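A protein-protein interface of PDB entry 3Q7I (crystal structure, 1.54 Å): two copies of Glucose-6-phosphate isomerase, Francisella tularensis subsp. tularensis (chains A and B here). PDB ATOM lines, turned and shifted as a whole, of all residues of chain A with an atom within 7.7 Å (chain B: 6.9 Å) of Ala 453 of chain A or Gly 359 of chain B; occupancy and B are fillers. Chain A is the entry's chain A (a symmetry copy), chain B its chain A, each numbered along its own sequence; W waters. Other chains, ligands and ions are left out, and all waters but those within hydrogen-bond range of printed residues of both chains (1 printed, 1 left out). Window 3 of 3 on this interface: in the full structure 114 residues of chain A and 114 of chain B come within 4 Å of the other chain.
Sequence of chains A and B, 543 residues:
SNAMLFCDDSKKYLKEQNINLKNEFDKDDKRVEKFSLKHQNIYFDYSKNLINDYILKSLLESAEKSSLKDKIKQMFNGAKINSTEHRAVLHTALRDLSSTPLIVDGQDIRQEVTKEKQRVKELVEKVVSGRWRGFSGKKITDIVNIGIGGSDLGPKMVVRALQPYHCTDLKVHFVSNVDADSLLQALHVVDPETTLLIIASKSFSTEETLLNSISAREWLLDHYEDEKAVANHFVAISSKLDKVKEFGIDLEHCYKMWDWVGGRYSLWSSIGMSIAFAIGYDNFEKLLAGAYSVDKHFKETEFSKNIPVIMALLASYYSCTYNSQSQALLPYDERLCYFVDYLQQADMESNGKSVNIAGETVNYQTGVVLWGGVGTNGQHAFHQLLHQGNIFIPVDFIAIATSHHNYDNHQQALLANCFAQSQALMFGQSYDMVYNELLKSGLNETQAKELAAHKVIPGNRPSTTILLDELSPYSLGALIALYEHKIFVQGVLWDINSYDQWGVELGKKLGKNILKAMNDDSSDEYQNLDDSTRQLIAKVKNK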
ATOM      1  N   GLN A 388      19.822   3.883  13.046  1.00  0.00           N
ATOM      2  CA  GLN A 388      19.380   5.272  12.992  1.00  0.00           C
ATOM      3  C   GLN A 388      18.385   5.730  14.018  1.00  0.00           C
ATOM      4  O   GLN A 388      17.968   6.897  13.974  1.00  0.00           O
ATOM      5  CB  GLN A 388      18.792   5.567  11.606  1.00  0.00           C
ATOM      6  CG  GLN A 388      19.800   5.633  10.447  1.00  0.00           C
ATOM      7  CD  GLN A 388      19.166   6.227   9.191  1.00  0.00           C
ATOM      8  OE1 GLN A 388      18.101   5.819   8.732  1.00  0.00           O
ATOM      9  NE2 GLN A 388      19.868   7.186   8.591  1.00  0.00           N
ATOM     10  N   GLN A 429      28.216   6.252   8.856  1.00  0.00           N
ATOM     11  CA  GLN A 429      28.468   6.993   7.600  1.00  0.00           C
ATOM     12  C   GLN A 429      28.195   8.468   7.858  1.00  0.00           C
ATOM     13  O   GLN A 429      27.067   8.832   8.228  1.00  0.00           O
ATOM     14  CB  GLN A 429      27.535   6.469   6.482  1.00  0.00           C
ATOM     15  CG  GLN A 429      27.890   5.079   5.896  1.00  0.00           C
ATOM     16  CD  GLN A 429      27.300   4.818   4.495  1.00  0.00           C
ATOM     17  OE1 GLN A 429      26.220   5.298   4.162  1.00  0.00           O
ATOM     18  NE2 GLN A 429      28.024   4.048   3.682  1.00  0.00           N
ATOM     19  N   TYR A 431      27.870  12.667   7.175  1.00  0.00           N
ATOM     20  CA  TYR A 431      27.269  13.567   6.197  1.00  0.00           C
ATOM     21  C   TYR A 431      28.158  13.727   4.965  1.00  0.00           C
ATOM     22  O   TYR A 431      27.688  13.616   3.826  1.00  0.00           O
ATOM     23  CB  TYR A 431      26.979  14.948   6.795  1.00  0.00           C
ATOM     24  CG  TYR A 431      26.278  15.898   5.858  1.00  0.00           C
ATOM     25  CD1 TYR A 431      24.894  16.052   5.898  1.00  0.00           C
ATOM     26  CD2 TYR A 431      26.994  16.683   4.966  1.00  0.00           C
ATOM     27  CE1 TYR A 431      24.233  16.916   5.031  1.00  0.00           C
ATOM     28  CE2 TYR A 431      26.332  17.568   4.113  1.00  0.00           C
ATOM     29  CZ  TYR A 431      24.955  17.664   4.155  1.00  0.00           C
ATOM     30  OH  TYR A 431      24.322  18.548   3.306  1.00  0.00           O
ATOM     31  N   VAL A 434      28.216  10.521   2.880  1.00  0.00           N
ATOM     32  CA  VAL A 434      26.928  10.349   2.207  1.00  0.00           C
ATOM     33  C   VAL A 434      26.737  11.349   1.068  1.00  0.00           C
ATOM     34  O   VAL A 434      26.339  10.975  -0.054  1.00  0.00           O
ATOM     35  CB  VAL A 434      25.757  10.470   3.209  1.00  0.00           C
ATOM     36  CG1 VAL A 434      24.446  10.732   2.400  1.00  0.00           C
ATOM     37  CG2 VAL A 434      25.732   9.234   4.103  1.00  0.00           C
ATOM     38  N   TYR A 435      27.000  12.621   1.343  1.00  0.00           N
ATOM     39  CA  TYR A 435      26.842  13.679   0.357  1.00  0.00           C
ATOM     40  C   TYR A 435      27.682  13.402  -0.900  1.00  0.00           C
ATOM     41  O   TYR A 435      27.181  13.475  -2.032  1.00  0.00           O
ATOM     42  CB  TYR A 435      27.240  14.994   0.983  1.00  0.00           C
ATOM     43  CG  TYR A 435      27.164  16.171   0.040  1.00  0.00           C
ATOM     44  CD1 TYR A 435      25.968  16.849  -0.167  1.00  0.00           C
ATOM     45  CD2 TYR A 435      28.297  16.614  -0.591  1.00  0.00           C
ATOM     46  CE1 TYR A 435      25.903  17.950  -1.018  1.00  0.00           C
ATOM     47  CE2 TYR A 435      28.252  17.718  -1.438  1.00  0.00           C
ATOM     48  CZ  TYR A 435      27.042  18.376  -1.650  1.00  0.00           C
ATOM     49  OH  TYR A 435      26.991  19.482  -2.500  1.00  0.00           O
ATOM     50  N   LEU A 438      26.224  10.672  -2.964  1.00  0.00           N
ATOM     51  CA  LEU A 438      25.009  11.075  -3.681  1.00  0.00           C
ATOM     52  C   LEU A 438      25.363  11.825  -4.945  1.00  0.00           C
ATOM     53  O   LEU A 438      24.747  11.595  -5.986  1.00  0.00           O
ATOM     54  CB  LEU A 438      24.094  11.947  -2.838  1.00  0.00           C
ATOM     55  CG  LEU A 438      23.378  11.227  -1.685  1.00  0.00           C
ATOM     56  CD1 LEU A 438      22.589  12.226  -0.851  1.00  0.00           C
ATOM     57  CD2 LEU A 438      22.492  10.093  -2.247  1.00  0.00           C
ATOM     58  N   ALA A 448      21.336  16.507  -3.368  1.00  0.00           N
ATOM     59  CA  ALA A 448      22.198  15.815  -2.417  1.00  0.00           C
ATOM     60  C   ALA A 448      22.103  16.467  -1.035  1.00  0.00           C
ATOM     61  O   ALA A 448      22.064  15.746  -0.012  1.00  0.00           O
ATOM     62  CB  ALA A 448      23.630  15.736  -2.880  1.00  0.00           C
ATOM     63  N   LYS A 449      22.014  17.795  -0.980  1.00  0.00           N
ATOM     64  CA  LYS A 449      21.881  18.502   0.303  1.00  0.00           C
ATOM     65  C   LYS A 449      20.568  18.184   1.007  1.00  0.00           C
ATOM     66  O   LYS A 449      20.528  18.093   2.234  1.00  0.00           O
ATOM     67  CB  LYS A 449      22.000  20.021   0.127  1.00  0.00           C
ATOM     68  CG  LYS A 449      21.717  20.783   1.425  1.00  0.00           C
ATOM     69  CD  LYS A 449      22.677  21.940   1.702  1.00  0.00           C
ATOM     70  CE  LYS A 449      22.708  22.220   3.210  1.00  0.00           C
ATOM     71  NZ  LYS A 449      21.329  22.191   3.794  1.00  0.00           N
ATOM     72  N   GLU A 450      19.500  18.016   0.232  1.00  0.00           N
ATOM     73  CA  GLU A 450      18.168  17.728   0.769  1.00  0.00           C
ATOM     74  C   GLU A 450      18.090  16.336   1.377  1.00  0.00           C
ATOM     75  O   GLU A 450      17.346  16.107   2.366  1.00  0.00           O
ATOM     76  CB  GLU A 450      17.129  17.801  -0.346  1.00  0.00           C
ATOM     77  CG  GLU A 450      15.877  18.571   0.019  1.00  0.00           C
ATOM     78  CD  GLU A 450      15.125  19.043  -1.206  1.00  0.00           C
ATOM     79  OE1 GLU A 450      15.313  20.217  -1.619  1.00  0.00           O
ATOM     80  OE2 GLU A 450      14.362  18.225  -1.762  1.00  0.00           O
ATOM     81  N   LEU A 451      18.821  15.409   0.771  1.00  0.00           N
ATOM     82  CA  LEU A 451      18.742  13.989   1.192  1.00  0.00           C
ATOM     83  C   LEU A 451      19.801  13.520   2.210  1.00  0.00           C
ATOM     84  O   LEU A 451      19.530  12.633   3.051  1.00  0.00           O
ATOM     85  CB  LEU A 451      18.789  13.108  -0.022  1.00  0.00           C
ATOM     86  CG  LEU A 451      18.733  11.621   0.148  1.00  0.00           C
ATOM     87  CD1 LEU A 451      17.409  11.282   0.955  1.00  0.00           C
ATOM     88  CD2 LEU A 451      18.773  10.878  -1.205  1.00  0.00           C
ATOM     89  N   ALA A 452      20.987  14.105   2.153  1.00  0.00           N
ATOM     90  CA  ALA A 452      22.113  13.558   2.858  1.00  0.00           C
ATOM     91  C   ALA A 452      21.871  13.361   4.350  1.00  0.00           C
ATOM     92  O   ALA A 452      22.272  12.336   4.871  1.00  0.00           O
ATOM     93  CB  ALA A 452      23.391  14.442   2.600  1.00  0.00           C
ATOM     94  N   ALA A 453      21.240  14.324   5.038  1.00  0.00           N
ATOM     95  CA  ALA A 453      21.095  14.210   6.485  1.00  0.00           C
ATOM     96  C   ALA A 453      20.278  12.993   6.831  1.00  0.00           C
ATOM     97  O   ALA A 453      20.513  12.397   7.888  1.00  0.00           O
ATOM     98  CB  ALA A 453      20.428  15.465   7.072  1.00  0.00           C
ATOM     99  N   HIS A 454      19.363  12.611   5.928  1.00  0.00           N
ATOM    100  CA  HIS A 454      18.483  11.437   6.202  1.00  0.00           C
ATOM    101  C   HIS A 454      19.214  10.128   6.087  1.00  0.00           C
ATOM    102  O   HIS A 454      18.767   9.148   6.643  1.00  0.00           O
ATOM    103  CB  HIS A 454      17.335  11.439   5.222  1.00  0.00           C
ATOM    104  CG  HIS A 454      16.434  12.605   5.390  1.00  0.00           C
ATOM    105  ND1 HIS A 454      15.435  12.650   6.340  1.00  0.00           N
ATOM    106  CD2 HIS A 454      16.480  13.834   4.829  1.00  0.00           C
ATOM    107  CE1 HIS A 454      14.857  13.827   6.297  1.00  0.00           C
ATOM    108  NE2 HIS A 454      15.482  14.584   5.397  1.00  0.00           N
ATOM    109  N   LYS A 455      20.344  10.102   5.393  1.00  0.00           N
ATOM    110  CA  LYS A 455      21.150   8.917   5.217  1.00  0.00           C
ATOM    111  C   LYS A 455      22.307   8.816   6.198  1.00  0.00           C
ATOM    112  O   LYS A 455      22.961   7.779   6.240  1.00  0.00           O
ATOM    113  CB  LYS A 455      21.699   8.827   3.821  1.00  0.00           C
ATOM    114  CG  LYS A 455      20.598   8.758   2.752  1.00  0.00           C
ATOM    115  CD  LYS A 455      21.092   8.462   1.383  1.00  0.00           C
ATOM    116  CE  LYS A 455      21.765   7.154   1.244  1.00  0.00           C
ATOM    117  NZ  LYS A 455      22.279   6.903  -0.162  1.00  0.00           N
ATOM    118  N   VAL A 456      22.553   9.876   6.992  1.00  0.00           N
ATOM    119  CA  VAL A 456      23.656   9.823   7.958  1.00  0.00           C
ATOM    120  C   VAL A 456      23.400   8.683   8.933  1.00  0.00           C
ATOM    121  O   VAL A 456      22.305   8.535   9.501  1.00  0.00           O
ATOM    122  CB  VAL A 456      23.847  11.157   8.666  1.00  0.00           C
ATOM    123  CG1 VAL A 456      24.779  11.020   9.885  1.00  0.00           C
ATOM    124  CG2 VAL A 456      24.429  12.153   7.667  1.00  0.00           C
ATOM    125  N   ILE A 457      24.440   7.896   9.197  1.00  0.00           N
ATOM    126  CA  ILE A 457      24.354   6.814  10.151  1.00  0.00           C
ATOM    127  C   ILE A 457      25.376   7.153  11.252  1.00  0.00           C
ATOM    128  O   ILE A 457      26.584   7.207  10.997  1.00  0.00           O
ATOM    129  CB  ILE A 457      24.733   5.481   9.520  1.00  0.00           C
ATOM    130  CG1 ILE A 457      23.990   5.170   8.210  1.00  0.00           C
ATOM    131  CG2 ILE A 457      24.586   4.320  10.585  1.00  0.00           C
ATOM    132  CD1 ILE A 457      22.668   4.794   8.341  1.00  0.00           C
ATOM    133  N   SER B 354      16.384   9.416  13.511  1.00  0.00           N
ATOM    134  CA  SER B 354      17.052  10.415  14.364  1.00  0.00           C
ATOM    135  C   SER B 354      16.897  11.836  13.854  1.00  0.00           C
ATOM    136  O   SER B 354      17.316  12.781  14.546  1.00  0.00           O
ATOM    137  CB  SER B 354      18.532  10.053  14.481  1.00  0.00           C
ATOM    138  OG  SER B 354      18.703   8.991  15.428  1.00  0.00           O
ATOM    139  N   VAL B 355      16.419  11.992  12.613  1.00  0.00           N
ATOM    140  CA  VAL B 355      16.189  13.305  12.034  1.00  0.00           C
ATOM    141  C   VAL B 355      14.738  13.491  11.691  1.00  0.00           C
ATOM    142  O   VAL B 355      14.007  12.539  11.434  1.00  0.00           O
ATOM    143  CB  VAL B 355      17.058  13.583  10.786  1.00  0.00           C
ATOM    144  CG1 VAL B 355      18.559  13.441  11.105  1.00  0.00           C
ATOM    145  CG2 VAL B 355      16.677  12.694   9.595  1.00  0.00           C
ATOM    146  N   ASN B 356      14.319  14.757  11.713  1.00  0.00           N
ATOM    147  CA  ASN B 356      12.980  15.130  11.304  1.00  0.00           C
ATOM    148  C   ASN B 356      12.867  15.278   9.782  1.00  0.00           C
ATOM    149  O   ASN B 356      13.833  15.029   9.039  1.00  0.00           O
ATOM    150  CB  ASN B 356      12.485  16.354  12.050  1.00  0.00           C
ATOM    151  CG  ASN B 356      13.313  17.569  11.788  1.00  0.00           C
ATOM    152  OD1 ASN B 356      13.964  17.698  10.734  1.00  0.00           O
ATOM    153  ND2 ASN B 356      13.194  18.572  12.700  1.00  0.00           N
ATOM    154  N   ILE B 357      11.674  15.636   9.325  1.00  0.00           N
ATOM    155  CA  ILE B 357      11.417  15.751   7.886  1.00  0.00           C
ATOM    156  C   ILE B 357      12.379  16.717   7.232  1.00  0.00           C
ATOM    157  O   ILE B 357      12.774  16.470   6.107  1.00  0.00           O
ATOM    158  CB  ILE B 357       9.972  16.190   7.626  1.00  0.00           C
ATOM    159  CG1 ILE B 357       8.986  15.114   8.106  1.00  0.00           C
ATOM    160  CG2 ILE B 357       9.737  16.540   6.162  1.00  0.00           C
ATOM    161  CD1 ILE B 357       9.132  13.855   7.439  1.00  0.00           C
ATOM    162  N   ALA B 358      12.774  17.775   7.947  1.00  0.00           N
ATOM    163  CA  ALA B 358      13.703  18.782   7.445  1.00  0.00           C
ATOM    164  C   ALA B 358      15.161  18.322   7.498  1.00  0.00           C
ATOM    165  O   ALA B 358      16.039  19.100   7.066  1.00  0.00           O
ATOM    166  CB  ALA B 358      13.511  20.104   8.200  1.00  0.00           C
ATOM    167  N   GLY B 359      15.450  17.139   8.040  1.00  0.00           N
ATOM    168  CA  GLY B 359      16.824  16.653   8.134  1.00  0.00           C
ATOM    169  C   GLY B 359      17.564  17.083   9.398  1.00  0.00           C
ATOM    170  O   GLY B 359      18.762  16.821   9.503  1.00  0.00           O
ATOM    171  N   GLU B 360      16.867  17.717  10.345  1.00  0.00           N
ATOM    172  CA  GLU B 360      17.487  18.167  11.563  1.00  0.00           C
ATOM    173  C   GLU B 360      17.527  17.040  12.577  1.00  0.00           C
ATOM    174  O   GLU B 360      16.532  16.328  12.753  1.00  0.00           O
ATOM    175  CB  GLU B 360      16.691  19.336  12.162  1.00  0.00           C
ATOM    176  CG  GLU B 360      16.553  20.526  11.199  1.00  0.00           C
ATOM    177  CD  GLU B 360      15.496  21.526  11.590  1.00  0.00           C
ATOM    178  OE1 GLU B 360      14.502  21.206  12.257  1.00  0.00           O
ATOM    179  OE2 GLU B 360      15.673  22.732  11.215  1.00  0.00           O
ATOM    180  N   THR B 361      18.635  16.904  13.288  1.00  0.00           N
ATOM    181  CA  THR B 361      18.750  15.923  14.351  1.00  0.00           C
ATOM    182  C   THR B 361      17.779  16.332  15.469  1.00  0.00           C
ATOM    183  O   THR B 361      17.850  17.482  15.994  1.00  0.00           O
ATOM    184  CB  THR B 361      20.196  15.849  14.866  1.00  0.00           C
ATOM    185  OG1 THR B 361      21.056  15.406  13.805  1.00  0.00           O
ATOM    186  CG2 THR B 361      20.284  14.835  16.051  1.00  0.00           C
ATOM    187  N   VAL B 362      16.904  15.439  15.885  1.00  0.00           N
ATOM    188  CA  VAL B 362      15.869  15.778  16.867  1.00  0.00           C
ATOM    189  C   VAL B 362      16.427  15.641  18.281  1.00  0.00           C
ATOM    190  O   VAL B 362      17.277  14.800  18.535  1.00  0.00           O
ATOM    191  CB  VAL B 362      14.553  14.971  16.715  1.00  0.00           C
ATOM    192  CG1 VAL B 362      13.928  15.245  15.316  1.00  0.00           C
ATOM    193  CG2 VAL B 362      14.750  13.449  16.952  1.00  0.00           C
HETATM  194  O   HOH W   1      17.890  17.841   4.894  1.00  0.00           O
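Of the printed residues of chain B, Ala 453 of chain A touches Val 355 and Gly 359.
Of the printed residues of chain A, Ser 354 of chain B touches Gln 388.
Of the printed residues of chain B, Gln 388 of chain A touches Ser 354 (2.7 Å).
Printed residues of chain A within 4 Å of Asn 356 of chain B: His 454 (3.2 Å).
Printed residues of chain B within 4 Å of His 454 of chain A: Val 355, Asn 356, Ile 357 and Gly 359.
Of the printed residues of chain A, Ile 357 of chain B touches His 454.
The nearest printed residue of chain A that does not touch Gly 359 of chain B is Glu 450 of chain A (5.8 Å).
The nearest printed residue of chain A that does not touch Asn 356 of chain B is Ala 453 of chain A (6.9 Å).
Water W1 bridges the backbone carbonyl oxygen (O) of Glu 450 of chain A (3.1 Å) and the backbone carbonyl oxygen (O) of Ala 358 of chain B (3.1 Å).
Ala 453 of chain A touches Val 355 of chain B (O to CG1, 3.9 Å).
Gly 359 of chain B touches Ala 453 of chain A.
ND1 of His 454 of chain A touches CG2 of Val 355 of chain B (3.5 Å).
CE1 of His 454 of chain A touches O of Asn 356 of chain B (3.2 Å).
His 454 of chain A touches Gly 359 of chain B (NE2 to N, 3.7 Å).
Of the 16 printed residues of chain A, 3 touch a printed residue of chain B.
Along chain B the printed residues that touch a printed residue of chain A span positions 354 to 359.
Among the printed residues, 7 pairs touch across the chains.
No position is printed for both chains.
Of the 7 pairs that touch across the chains among the printed residues, none has its exchanged pair printed and touching as well.
The side-chain amide oxygen of Asn 356 of chain B sits at hydrogen-bond distance from the backbone NH of Gly 359 of chain B, 3.1 Å away.
The backbone carbonyl oxygen (O) of Ser 354 of chain B sits at hydrogen-bond distance from the backbone NH (N) of Val 362 of chain B.
The side-chain amide oxygen (OD1) of Asn 356 of chain B sits at hydrogen-bond distance from the backbone NH (N) of Ala 358 of chain B (3.0 Å).
The side-chain amide nitrogen (NE2) of Gln 388 of chain A is in hydrogen-bond range of the backbone carbonyl oxygen (O) of Val 456 of chain A (2.9 Å).
The backbone NH of Glu 360 of chain B is in hydrogen-bond range of the side-chain amide oxygen of Asn 356 of chain B.
The side-chain amide nitrogen of Gln 388 of chain A lies within hydrogen-bond range of the backbone carbonyl oxygen of His 454 of chain A (3.0 Å).
The side-chain hydroxyl (OG) of Ser 354 of chain B lies within hydrogen-bond range of the backbone carbonyl oxygen (O) of Gln 388 of chain A (2.7 Å).
O of Ile 357 of chain B sits close to NE2 of His 454 of chain A (3.4 Å).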
